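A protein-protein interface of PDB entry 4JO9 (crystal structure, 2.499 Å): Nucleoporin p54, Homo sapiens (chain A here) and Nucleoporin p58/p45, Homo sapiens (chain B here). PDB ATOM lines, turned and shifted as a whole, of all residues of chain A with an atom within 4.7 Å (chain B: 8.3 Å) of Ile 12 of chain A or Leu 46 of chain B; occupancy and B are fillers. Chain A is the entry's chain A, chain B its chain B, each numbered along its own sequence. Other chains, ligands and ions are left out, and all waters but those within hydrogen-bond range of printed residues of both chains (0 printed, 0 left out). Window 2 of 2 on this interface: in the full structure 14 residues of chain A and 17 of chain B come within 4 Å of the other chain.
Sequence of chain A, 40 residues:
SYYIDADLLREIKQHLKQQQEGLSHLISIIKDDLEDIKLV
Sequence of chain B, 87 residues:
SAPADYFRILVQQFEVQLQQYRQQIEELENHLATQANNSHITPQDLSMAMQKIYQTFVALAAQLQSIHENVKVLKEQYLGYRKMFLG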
ATOM      1  N   ILE A   4      17.446 -24.749  11.829  1.00  0.00           N
ATOM      2  CA  ILE A   4      16.595 -23.940  12.698  1.00  0.00           C
ATOM      3  C   ILE A   4      16.637 -24.397  14.152  1.00  0.00           C
ATOM      4  O   ILE A   4      16.970 -25.545  14.450  1.00  0.00           O
ATOM      5  CB  ILE A   4      15.130 -23.983  12.214  1.00  0.00           C
ATOM      6  CG1 ILE A   4      14.326 -22.829  12.819  1.00  0.00           C
ATOM      7  CG2 ILE A   4      14.494 -25.331  12.546  1.00  0.00           C
ATOM      8  CD1 ILE A   4      12.915 -22.736  12.287  1.00  0.00           C
ATOM      9  N   LEU A   8      11.992 -24.371  18.617  1.00  0.00           N
ATOM     10  CA  LEU A   8      10.981 -23.950  17.656  1.00  0.00           C
ATOM     11  C   LEU A   8      10.487 -25.150  16.855  1.00  0.00           C
ATOM     12  O   LEU A   8       9.364 -25.153  16.351  1.00  0.00           O
ATOM     13  CB  LEU A   8      11.546 -22.878  16.723  1.00  0.00           C
ATOM     14  CG  LEU A   8      10.575 -22.257  15.717  1.00  0.00           C
ATOM     15  CD1 LEU A   8       9.259 -21.879  16.380  1.00  0.00           C
ATOM     16  CD2 LEU A   8      11.209 -21.036  15.071  1.00  0.00           C
ATOM     17  N   LEU A   9      11.329 -26.172  16.743  1.00  0.00           N
ATOM     18  CA  LEU A   9      10.944 -27.404  16.067  1.00  0.00           C
ATOM     19  C   LEU A   9       9.928 -28.171  16.906  1.00  0.00           C
ATOM     20  O   LEU A   9       8.900 -28.613  16.396  1.00  0.00           O
ATOM     21  CB  LEU A   9      12.176 -28.272  15.800  1.00  0.00           C
ATOM     22  CG  LEU A   9      11.922 -29.639  15.160  1.00  0.00           C
ATOM     23  CD1 LEU A   9      13.145 -30.088  14.379  1.00  0.00           C
ATOM     24  CD2 LEU A   9      11.562 -30.687  16.207  1.00  0.00           C
ATOM     25  N   ARG A  10      10.224 -28.329  18.192  1.00  0.00           N
ATOM     26  CA  ARG A  10       9.324 -29.026  19.104  1.00  0.00           C
ATOM     27  C   ARG A  10       7.988 -28.299  19.209  1.00  0.00           C
ATOM     28  O   ARG A  10       6.950 -28.919  19.437  1.00  0.00           O
ATOM     29  CB  ARG A  10       9.967 -29.163  20.488  1.00  0.00           C
ATOM     30  CG  ARG A  10      10.995 -30.281  20.570  1.00  0.00           C
ATOM     31  CD  ARG A  10      12.261 -29.847  21.296  1.00  0.00           C
ATOM     32  NE  ARG A  10      12.098 -29.805  22.746  1.00  0.00           N
ATOM     33  CZ  ARG A  10      13.074 -29.509  23.598  1.00  0.00           C
ATOM     34  NH1 ARG A  10      14.289 -29.226  23.149  1.00  0.00           N
ATOM     35  NH2 ARG A  10      12.837 -29.495  24.902  1.00  0.00           N
ATOM     36  N   GLU A  11       8.021 -26.982  19.040  1.00  0.00           N
ATOM     37  CA  GLU A  11       6.804 -26.181  19.056  1.00  0.00           C
ATOM     38  C   GLU A  11       5.967 -26.465  17.814  1.00  0.00           C
ATOM     39  O   GLU A  11       4.758 -26.678  17.904  1.00  0.00           O
ATOM     40  CB  GLU A  11       7.150 -24.693  19.132  1.00  0.00           C
ATOM     41  CG  GLU A  11       7.683 -24.254  20.486  1.00  0.00           C
ATOM     42  CD  GLU A  11       8.356 -22.896  20.438  1.00  0.00           C
ATOM     43  OE1 GLU A  11       8.982 -22.505  21.446  1.00  0.00           O
ATOM     44  OE2 GLU A  11       8.257 -22.218  19.393  1.00  0.00           O
ATOM     45  N   ILE A  12       6.619 -26.469  16.656  1.00  0.00           N
ATOM     46  CA  ILE A  12       5.946 -26.756  15.397  1.00  0.00           C
ATOM     47  C   ILE A  12       5.373 -28.170  15.401  1.00  0.00           C
ATOM     48  O   ILE A  12       4.210 -28.373  15.057  1.00  0.00           O
ATOM     49  CB  ILE A  12       6.905 -26.598  14.203  1.00  0.00           C
ATOM     50  CG1 ILE A  12       7.253 -25.122  14.001  1.00  0.00           C
ATOM     51  CG2 ILE A  12       6.278 -27.164  12.935  1.00  0.00           C
ATOM     52  CD1 ILE A  12       8.359 -24.880  12.994  1.00  0.00           C
ATOM     53  N   LYS A  13       6.191 -29.142  15.792  1.00  0.00           N
ATOM     54  CA  LYS A  13       5.751 -30.532  15.851  1.00  0.00           C
ATOM     55  C   LYS A  13       4.521 -30.680  16.739  1.00  0.00           C
ATOM     56  O   LYS A  13       3.581 -31.395  16.397  1.00  0.00           O
ATOM     57  CB  LYS A  13       6.875 -31.436  16.363  1.00  0.00           C
ATOM     58  CG  LYS A  13       7.573 -32.223  15.268  1.00  0.00           C
ATOM     59  CD  LYS A  13       8.756 -33.006  15.811  1.00  0.00           C
ATOM     60  CE  LYS A  13       9.678 -33.454  14.690  1.00  0.00           C
ATOM     61  NZ  LYS A  13      10.828 -34.254  15.193  1.00  0.00           N
ATOM     62  N   GLN A  14       4.529 -29.997  17.879  1.00  0.00           N
ATOM     63  CA  GLN A  14       3.410 -30.056  18.810  1.00  0.00           C
ATOM     64  C   GLN A  14       2.155 -29.457  18.185  1.00  0.00           C
ATOM     65  O   GLN A  14       1.049 -29.948  18.405  1.00  0.00           O
ATOM     66  CB  GLN A  14       3.752 -29.309  20.100  1.00  0.00           C
ATOM     67  CG  GLN A  14       2.619 -29.260  21.113  1.00  0.00           C
ATOM     68  CD  GLN A  14       2.078 -30.632  21.487  1.00  0.00           C
ATOM     69  OE1 GLN A  14       0.922 -30.757  21.894  1.00  0.00           O
ATOM     70  NE2 GLN A  14       2.909 -31.663  21.363  1.00  0.00           N
ATOM     71  N   HIS A  15       2.333 -28.391  17.412  1.00  0.00           N
ATOM     72  CA  HIS A  15       1.213 -27.705  16.783  1.00  0.00           C
ATOM     73  C   HIS A  15       0.572 -28.576  15.709  1.00  0.00           C
ATOM     74  O   HIS A  15      -0.644 -28.762  15.695  1.00  0.00           O
ATOM     75  CB  HIS A  15       1.670 -26.382  16.168  1.00  0.00           C
ATOM     76  CG  HIS A  15       0.556 -25.583  15.566  1.00  0.00           C
ATOM     77  ND1 HIS A  15      -0.477 -25.063  16.317  1.00  0.00           N
ATOM     78  CD2 HIS A  15       0.311 -25.217  14.285  1.00  0.00           C
ATOM     79  CE1 HIS A  15      -1.308 -24.410  15.525  1.00  0.00           C
ATOM     80  NE2 HIS A  15      -0.853 -24.489  14.288  1.00  0.00           N
ATOM     81  N   LEU A  16       1.395 -29.103  14.809  1.00  0.00           N
ATOM     82  CA  LEU A  16       0.909 -29.960  13.737  1.00  0.00           C
ATOM     83  C   LEU A  16       0.243 -31.204  14.311  1.00  0.00           C
ATOM     84  O   LEU A  16      -0.755 -31.690  13.777  1.00  0.00           O
ATOM     85  CB  LEU A  16       2.055 -30.360  12.807  1.00  0.00           C
ATOM     86  CG  LEU A  16       2.765 -29.209  12.091  1.00  0.00           C
ATOM     87  CD1 LEU A  16       3.780 -29.747  11.095  1.00  0.00           C
ATOM     88  CD2 LEU A  16       1.766 -28.291  11.399  1.00  0.00           C
ATOM     89  N   GLU B  27       5.657 -31.185   2.208  1.00  0.00           N
ATOM     90  CA  GLU B  27       6.616 -30.152   1.842  1.00  0.00           C
ATOM     91  C   GLU B  27       7.319 -29.607   3.079  1.00  0.00           C
ATOM     92  O   GLU B  27       8.507 -29.286   3.039  1.00  0.00           O
ATOM     93  CB  GLU B  27       5.918 -29.009   1.101  1.00  0.00           C
ATOM     94  CG  GLU B  27       5.589 -29.312  -0.350  1.00  0.00           C
ATOM     95  CD  GLU B  27       6.828 -29.404  -1.222  1.00  0.00           C
ATOM     96  OE1 GLU B  27       6.682 -29.628  -2.442  1.00  0.00           O
ATOM     97  OE2 GLU B  27       7.948 -29.250  -0.688  1.00  0.00           O
ATOM     98  N   LEU B  28       6.577 -29.505   4.176  1.00  0.00           N
ATOM     99  CA  LEU B  28       7.113 -28.943   5.409  1.00  0.00           C
ATOM    100  C   LEU B  28       7.971 -29.958   6.156  1.00  0.00           C
ATOM    101  O   LEU B  28       9.066 -29.636   6.613  1.00  0.00           O
ATOM    102  CB  LEU B  28       5.974 -28.460   6.307  1.00  0.00           C
ATOM    103  CG  LEU B  28       6.394 -27.659   7.540  1.00  0.00           C
ATOM    104  CD1 LEU B  28       7.202 -26.434   7.142  1.00  0.00           C
ATOM    105  CD2 LEU B  28       5.173 -27.252   8.344  1.00  0.00           C
ATOM    106  N   GLU B  29       7.470 -31.183   6.279  1.00  0.00           N
ATOM    107  CA  GLU B  29       8.210 -32.243   6.951  1.00  0.00           C
ATOM    108  C   GLU B  29       9.572 -32.446   6.298  1.00  0.00           C
ATOM    109  O   GLU B  29      10.579 -32.607   6.985  1.00  0.00           O
ATOM    110  CB  GLU B  29       7.419 -33.552   6.926  1.00  0.00           C
ATOM    111  CG  GLU B  29       6.205 -33.559   7.839  1.00  0.00           C
ATOM    112  CD  GLU B  29       5.496 -34.899   7.851  1.00  0.00           C
ATOM    113  OE1 GLU B  29       4.656 -35.120   8.747  1.00  0.00           O
ATOM    114  OE2 GLU B  29       5.780 -35.731   6.963  1.00  0.00           O
ATOM    115  N   HIS B  31      11.293 -30.251   4.596  1.00  0.00           N
ATOM    116  CA  HIS B  31      12.120 -29.089   4.893  1.00  0.00           C
ATOM    117  C   HIS B  31      12.735 -29.190   6.284  1.00  0.00           C
ATOM    118  O   HIS B  31      13.899 -28.845   6.483  1.00  0.00           O
ATOM    119  CB  HIS B  31      11.294 -27.808   4.794  1.00  0.00           C
ATOM    120  CG  HIS B  31      10.972 -27.400   3.390  1.00  0.00           C
ATOM    121  ND1 HIS B  31      11.557 -27.986   2.288  1.00  0.00           N
ATOM    122  CD2 HIS B  31      10.123 -26.461   2.911  1.00  0.00           C
ATOM    123  CE1 HIS B  31      11.083 -27.424   1.190  1.00  0.00           C
ATOM    124  NE2 HIS B  31      10.210 -26.496   1.540  1.00  0.00           N
ATOM    125  N   LEU B  32      11.946 -29.659   7.244  1.00  0.00           N
ATOM    126  CA  LEU B  32      12.407 -29.773   8.621  1.00  0.00           C
ATOM    127  C   LEU B  32      13.030 -31.140   8.895  1.00  0.00           C
ATOM    128  O   LEU B  32      13.455 -31.420  10.015  1.00  0.00           O
ATOM    129  CB  LEU B  32      11.245 -29.541   9.587  1.00  0.00           C
ATOM    130  CG  LEU B  32      10.465 -28.240   9.389  1.00  0.00           C
ATOM    131  CD1 LEU B  32       9.305 -28.160  10.370  1.00  0.00           C
ATOM    132  CD2 LEU B  32      11.376 -27.032   9.531  1.00  0.00           C
ATOM    133  N   ASN B  37      18.486 -29.353   4.730  1.00  0.00           N
ATOM    134  CA  ASN B  37      17.230 -29.009   4.064  1.00  0.00           C
ATOM    135  C   ASN B  37      16.641 -27.703   4.585  1.00  0.00           C
ATOM    136  O   ASN B  37      16.091 -26.912   3.819  1.00  0.00           O
ATOM    137  CB  ASN B  37      16.213 -30.142   4.219  1.00  0.00           C
ATOM    138  CG  ASN B  37      16.600 -31.383   3.440  1.00  0.00           C
ATOM    139  OD1 ASN B  37      17.730 -31.505   2.967  1.00  0.00           O
ATOM    140  ND2 ASN B  37      15.664 -32.316   3.306  1.00  0.00           N
ATOM    141  N   ASN B  38      16.757 -27.481   5.891  1.00  0.00           N
ATOM    142  CA  ASN B  38      16.259 -26.256   6.503  1.00  0.00           C
ATOM    143  C   ASN B  38      17.065 -25.052   6.029  1.00  0.00           C
ATOM    144  O   ASN B  38      16.548 -23.938   5.950  1.00  0.00           O
ATOM    145  CB  ASN B  38      16.323 -26.360   8.028  1.00  0.00           C
ATOM    146  CG  ASN B  38      15.393 -25.378   8.724  1.00  0.00           C
ATOM    147  OD1 ASN B  38      14.474 -25.781   9.436  1.00  0.00           O
ATOM    148  ND2 ASN B  38      15.630 -24.085   8.525  1.00  0.00           N
ATOM    149  N   HIS B  40      18.006 -24.461   3.175  1.00  0.00           N
ATOM    150  CA  HIS B  40      17.557 -24.063   1.845  1.00  0.00           C
ATOM    151  C   HIS B  40      16.264 -23.250   1.889  1.00  0.00           C
ATOM    152  O   HIS B  40      15.692 -22.930   0.848  1.00  0.00           O
ATOM    153  CB  HIS B  40      17.372 -25.292   0.952  1.00  0.00           C
ATOM    154  CG  HIS B  40      18.659 -25.882   0.463  1.00  0.00           C
ATOM    155  ND1 HIS B  40      19.513 -25.207  -0.382  1.00  0.00           N
ATOM    156  CD2 HIS B  40      19.234 -27.086   0.696  1.00  0.00           C
ATOM    157  CE1 HIS B  40      20.561 -25.968  -0.645  1.00  0.00           C
ATOM    158  NE2 HIS B  40      20.416 -27.113  -0.004  1.00  0.00           N
ATOM    159  N   ILE B  41      15.808 -22.915   3.093  1.00  0.00           N
ATOM    160  CA  ILE B  41      14.628 -22.073   3.251  1.00  0.00           C
ATOM    161  C   ILE B  41      14.819 -21.084   4.396  1.00  0.00           C
ATOM    162  O   ILE B  41      15.531 -21.363   5.359  1.00  0.00           O
ATOM    163  CB  ILE B  41      13.359 -22.908   3.512  1.00  0.00           C
ATOM    164  CG1 ILE B  41      13.535 -23.770   4.763  1.00  0.00           C
ATOM    165  CG2 ILE B  41      13.038 -23.774   2.302  1.00  0.00           C
ATOM    166  CD1 ILE B  41      12.273 -24.475   5.192  1.00  0.00           C
ATOM    167  N   THR B  42      14.178 -19.927   4.277  1.00  0.00           N
ATOM    168  CA  THR B  42      14.282 -18.877   5.280  1.00  0.00           C
ATOM    169  C   THR B  42      13.234 -19.089   6.368  1.00  0.00           C
ATOM    170  O   THR B  42      12.247 -19.792   6.152  1.00  0.00           O
ATOM    171  CB  THR B  42      14.087 -17.492   4.638  1.00  0.00           C
ATOM    172  OG1 THR B  42      12.791 -17.415   4.033  1.00  0.00           O
ATOM    173  CG2 THR B  42      15.142 -17.249   3.574  1.00  0.00           C
ATOM    174  N   PRO B  43      13.443 -18.483   7.547  1.00  0.00           N
ATOM    175  CA  PRO B  43      12.464 -18.646   8.627  1.00  0.00           C
ATOM    176  C   PRO B  43      11.094 -18.090   8.252  1.00  0.00           C
ATOM    177  O   PRO B  43      10.090 -18.481   8.845  1.00  0.00           O
ATOM    178  CB  PRO B  43      13.076 -17.842   9.781  1.00  0.00           C
ATOM    179  CG  PRO B  43      14.011 -16.884   9.132  1.00  0.00           C
ATOM    180  CD  PRO B  43      14.555 -17.602   7.940  1.00  0.00           C
ATOM    181  N   GLN B  44      11.058 -17.191   7.274  1.00  0.00           N
ATOM    182  CA  GLN B  44       9.804 -16.587   6.841  1.00  0.00           C
ATOM    183  C   GLN B  44       9.084 -17.459   5.810  1.00  0.00           C
ATOM    184  O   GLN B  44       7.951 -17.168   5.424  1.00  0.00           O
ATOM    185  CB  GLN B  44      10.055 -15.188   6.277  1.00  0.00           C
ATOM    186  CG  GLN B  44       9.172 -14.113   6.891  1.00  0.00           C
ATOM    187  CD  GLN B  44       9.626 -12.714   6.526  1.00  0.00           C
ATOM    188  OE1 GLN B  44      10.815 -12.401   6.585  1.00  0.00           O
ATOM    189  NE2 GLN B  44       8.678 -11.863   6.144  1.00  0.00           N
ATOM    190  N   ASP B  45       9.743 -18.525   5.364  1.00  0.00           N
ATOM    191  CA  ASP B  45       9.091 -19.515   4.516  1.00  0.00           C
ATOM    192  C   ASP B  45       8.237 -20.401   5.407  1.00  0.00           C
ATOM    193  O   ASP B  45       7.098 -20.729   5.074  1.00  0.00           O
ATOM    194  CB  ASP B  45      10.117 -20.361   3.760  1.00  0.00           C
ATOM    195  CG  ASP B  45      10.836 -19.578   2.681  1.00  0.00           C
ATOM    196  OD1 ASP B  45      10.336 -18.503   2.292  1.00  0.00           O
ATOM    197  OD2 ASP B  45      11.899 -20.042   2.215  1.00  0.00           O
ATOM    198  N   LEU B  46       8.802 -20.782   6.548  1.00  0.00           N
ATOM    199  CA  LEU B  46       8.057 -21.515   7.561  1.00  0.00           C
ATOM    200  C   LEU B  46       6.822 -20.722   7.962  1.00  0.00           C
ATOM    201  O   LEU B  46       5.710 -21.244   7.943  1.00  0.00           O
ATOM    202  CB  LEU B  46       8.932 -21.770   8.790  1.00  0.00           C
ATOM    203  CG  LEU B  46       9.561 -23.161   8.893  1.00  0.00           C
ATOM    204  CD1 LEU B  46      10.378 -23.488   7.653  1.00  0.00           C
ATOM    205  CD2 LEU B  46      10.421 -23.255  10.145  1.00  0.00           C
ATOM    206  N   SER B  47       7.024 -19.457   8.320  1.00  0.00           N
ATOM    207  CA  SER B  47       5.923 -18.593   8.730  1.00  0.00           C
ATOM    208  C   SER B  47       4.797 -18.623   7.700  1.00  0.00           C
ATOM    209  O   SER B  47       3.625 -18.484   8.046  1.00  0.00           O
ATOM    210  CB  SER B  47       6.415 -17.157   8.924  1.00  0.00           C
ATOM    211  OG  SER B  47       5.378 -16.329   9.420  1.00  0.00           O
ATOM    212  N   MET B  48       5.163 -18.799   6.434  1.00  0.00           N
ATOM    213  CA  MET B  48       4.179 -18.944   5.368  1.00  0.00           C
ATOM    214  C   MET B  48       3.525 -20.316   5.445  1.00  0.00           C
ATOM    215  O   MET B  48       2.319 -20.429   5.660  1.00  0.00           O
ATOM    216  CB  MET B  48       4.839 -18.772   3.998  1.00  0.00           C
ATOM    217  CG  MET B  48       4.499 -17.470   3.291  1.00  0.00           C
ATOM    218  SD  MET B  48       2.805 -17.409   2.673  1.00  0.00           S
ATOM    219  CE  MET B  48       2.018 -16.355   3.893  1.00  0.00           C
ATOM    220  N   ALA B  49       4.335 -21.355   5.266  1.00  0.00           N
ATOM    221  CA  ALA B  49       3.860 -22.731   5.313  1.00  0.00           C
ATOM    222  C   ALA B  49       2.927 -22.959   6.500  1.00  0.00           C
ATOM    223  O   ALA B  49       1.844 -23.520   6.348  1.00  0.00           O
ATOM    224  CB  ALA B  49       5.039 -23.688   5.378  1.00  0.00           C
ATOM    225  N   MET B  50       3.353 -22.521   7.679  1.00  0.00           N
ATOM    226  CA  MET B  50       2.556 -22.679   8.890  1.00  0.00           C
ATOM    227  C   MET B  50       1.175 -22.055   8.719  1.00  0.00           C
ATOM    228  O   MET B  50       0.160 -22.687   9.013  1.00  0.00           O
ATOM    229  CB  MET B  50       3.266 -22.039  10.086  1.00  0.00           C
ATOM    230  CG  MET B  50       4.548 -22.744  10.508  1.00  0.00           C
ATOM    231  SD  MET B  50       4.317 -24.503  10.828  1.00  0.00           S
ATOM    232  CE  MET B  50       3.017 -24.461  12.059  1.00  0.00           C
ATOM    233  N   GLN B  51       1.142 -20.815   8.245  1.00  0.00           N
ATOM    234  CA  GLN B  51      -0.117 -20.099   8.061  1.00  0.00           C
ATOM    235  C   GLN B  51      -0.948 -20.697   6.929  1.00  0.00           C
ATOM    236  O   GLN B  51      -2.169 -20.554   6.909  1.00  0.00           O
ATOM    237  CB  GLN B  51       0.147 -18.616   7.790  1.00  0.00           C
ATOM    238  CG  GLN B  51       0.517 -17.817   9.031  1.00  0.00           C
ATOM    239  CD  GLN B  51      -0.659 -17.616   9.969  1.00  0.00           C
ATOM    240  OE1 GLN B  51      -0.669 -18.124  11.092  1.00  0.00           O
ATOM    241  NE2 GLN B  51      -1.657 -16.868   9.515  1.00  0.00           N
ATOM    242  N   LYS B  52      -0.286 -21.368   5.992  1.00  0.00           N
ATOM    243  CA  LYS B  52      -0.979 -22.009   4.881  1.00  0.00           C
ATOM    244  C   LYS B  52      -1.620 -23.318   5.326  1.00  0.00           C
ATOM    245  O   LYS B  52      -2.780 -23.589   5.016  1.00  0.00           O
ATOM    246  CB  LYS B  52      -0.014 -22.271   3.723  1.00  0.00           C
ATOM    247  CG  LYS B  52       0.438 -21.020   2.990  1.00  0.00           C
ATOM    248  CD  LYS B  52      -0.742 -20.258   2.406  1.00  0.00           C
ATOM    249  CE  LYS B  52      -0.293 -19.039   1.620  1.00  0.00           C
ATOM    250  NZ  LYS B  52       0.491 -19.406   0.410  1.00  0.00           N
ATOM    251  N   ILE B  53      -0.858 -24.124   6.056  1.00  0.00           N
ATOM    252  CA  ILE B  53      -1.348 -25.407   6.540  1.00  0.00           C
ATOM    253  C   ILE B  53      -2.501 -25.209   7.514  1.00  0.00           C
ATOM    254  O   ILE B  53      -3.422 -26.023   7.571  1.00  0.00           O
ATOM    255  CB  ILE B  53      -0.239 -26.205   7.241  1.00  0.00           C
ATOM    256  CG1 ILE B  53       0.866 -26.563   6.248  1.00  0.00           C
ATOM    257  CG2 ILE B  53      -0.805 -27.476   7.855  1.00  0.00           C
ATOM    258  CD1 ILE B  53       2.119 -27.097   6.902  1.00  0.00           C
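N of Asn 38 of chain B is in hydrogen-bond range of O of His 31 of chain B.
Among the printed residues, pairs that only touch across the chains: Ile 4 of chain A with Asn 38 of chain B, Ile 4 of chain A with Leu 46 of chain B, Ile 12 of chain A with Leu 46 of chain B, Ile 12 of chain A with Met 50 of chain B, His 15 of chain A with Met 50 of chain B and Leu 16 of chain A with Leu 28 of chain B.
Of chain A, only Ile 4 (3.3 Å) and Ile 12 (3.9 Å) come within 4 Å of Leu 46 of chain B.
Printed residues of chain B within 4 Å of Ile 4 of chain A: Asn 38 (3.1 Å) and Leu 46 (3.3 Å).
Printed residues of chain A within 4 Å of Met 50 of chain B: Ile 12 and His 15.
Of the printed residues of chain B, His 15 of chain A touches Met 50 (3.6 Å).
Printed residues of chain A within 4 Å of Leu 28 of chain B: Leu 16.
Ile 53 of chain B touches none of the printed residues of chain A.
The nearest printed residue of chain A that does not touch Leu 46 of chain B is Leu 8 of chain A (5.5 Å).
Of the 21 printed residues of chain B, 4 touch a printed residue of chain A.
Along chain B the printed residues that touch a printed residue of chain A span positions 28 to 50.
Of the 10 printed residues of chain A, 4 touch a printed residue of chain B.
Along chain A the printed residues that touch a printed residue of chain B span positions 4 to 16.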
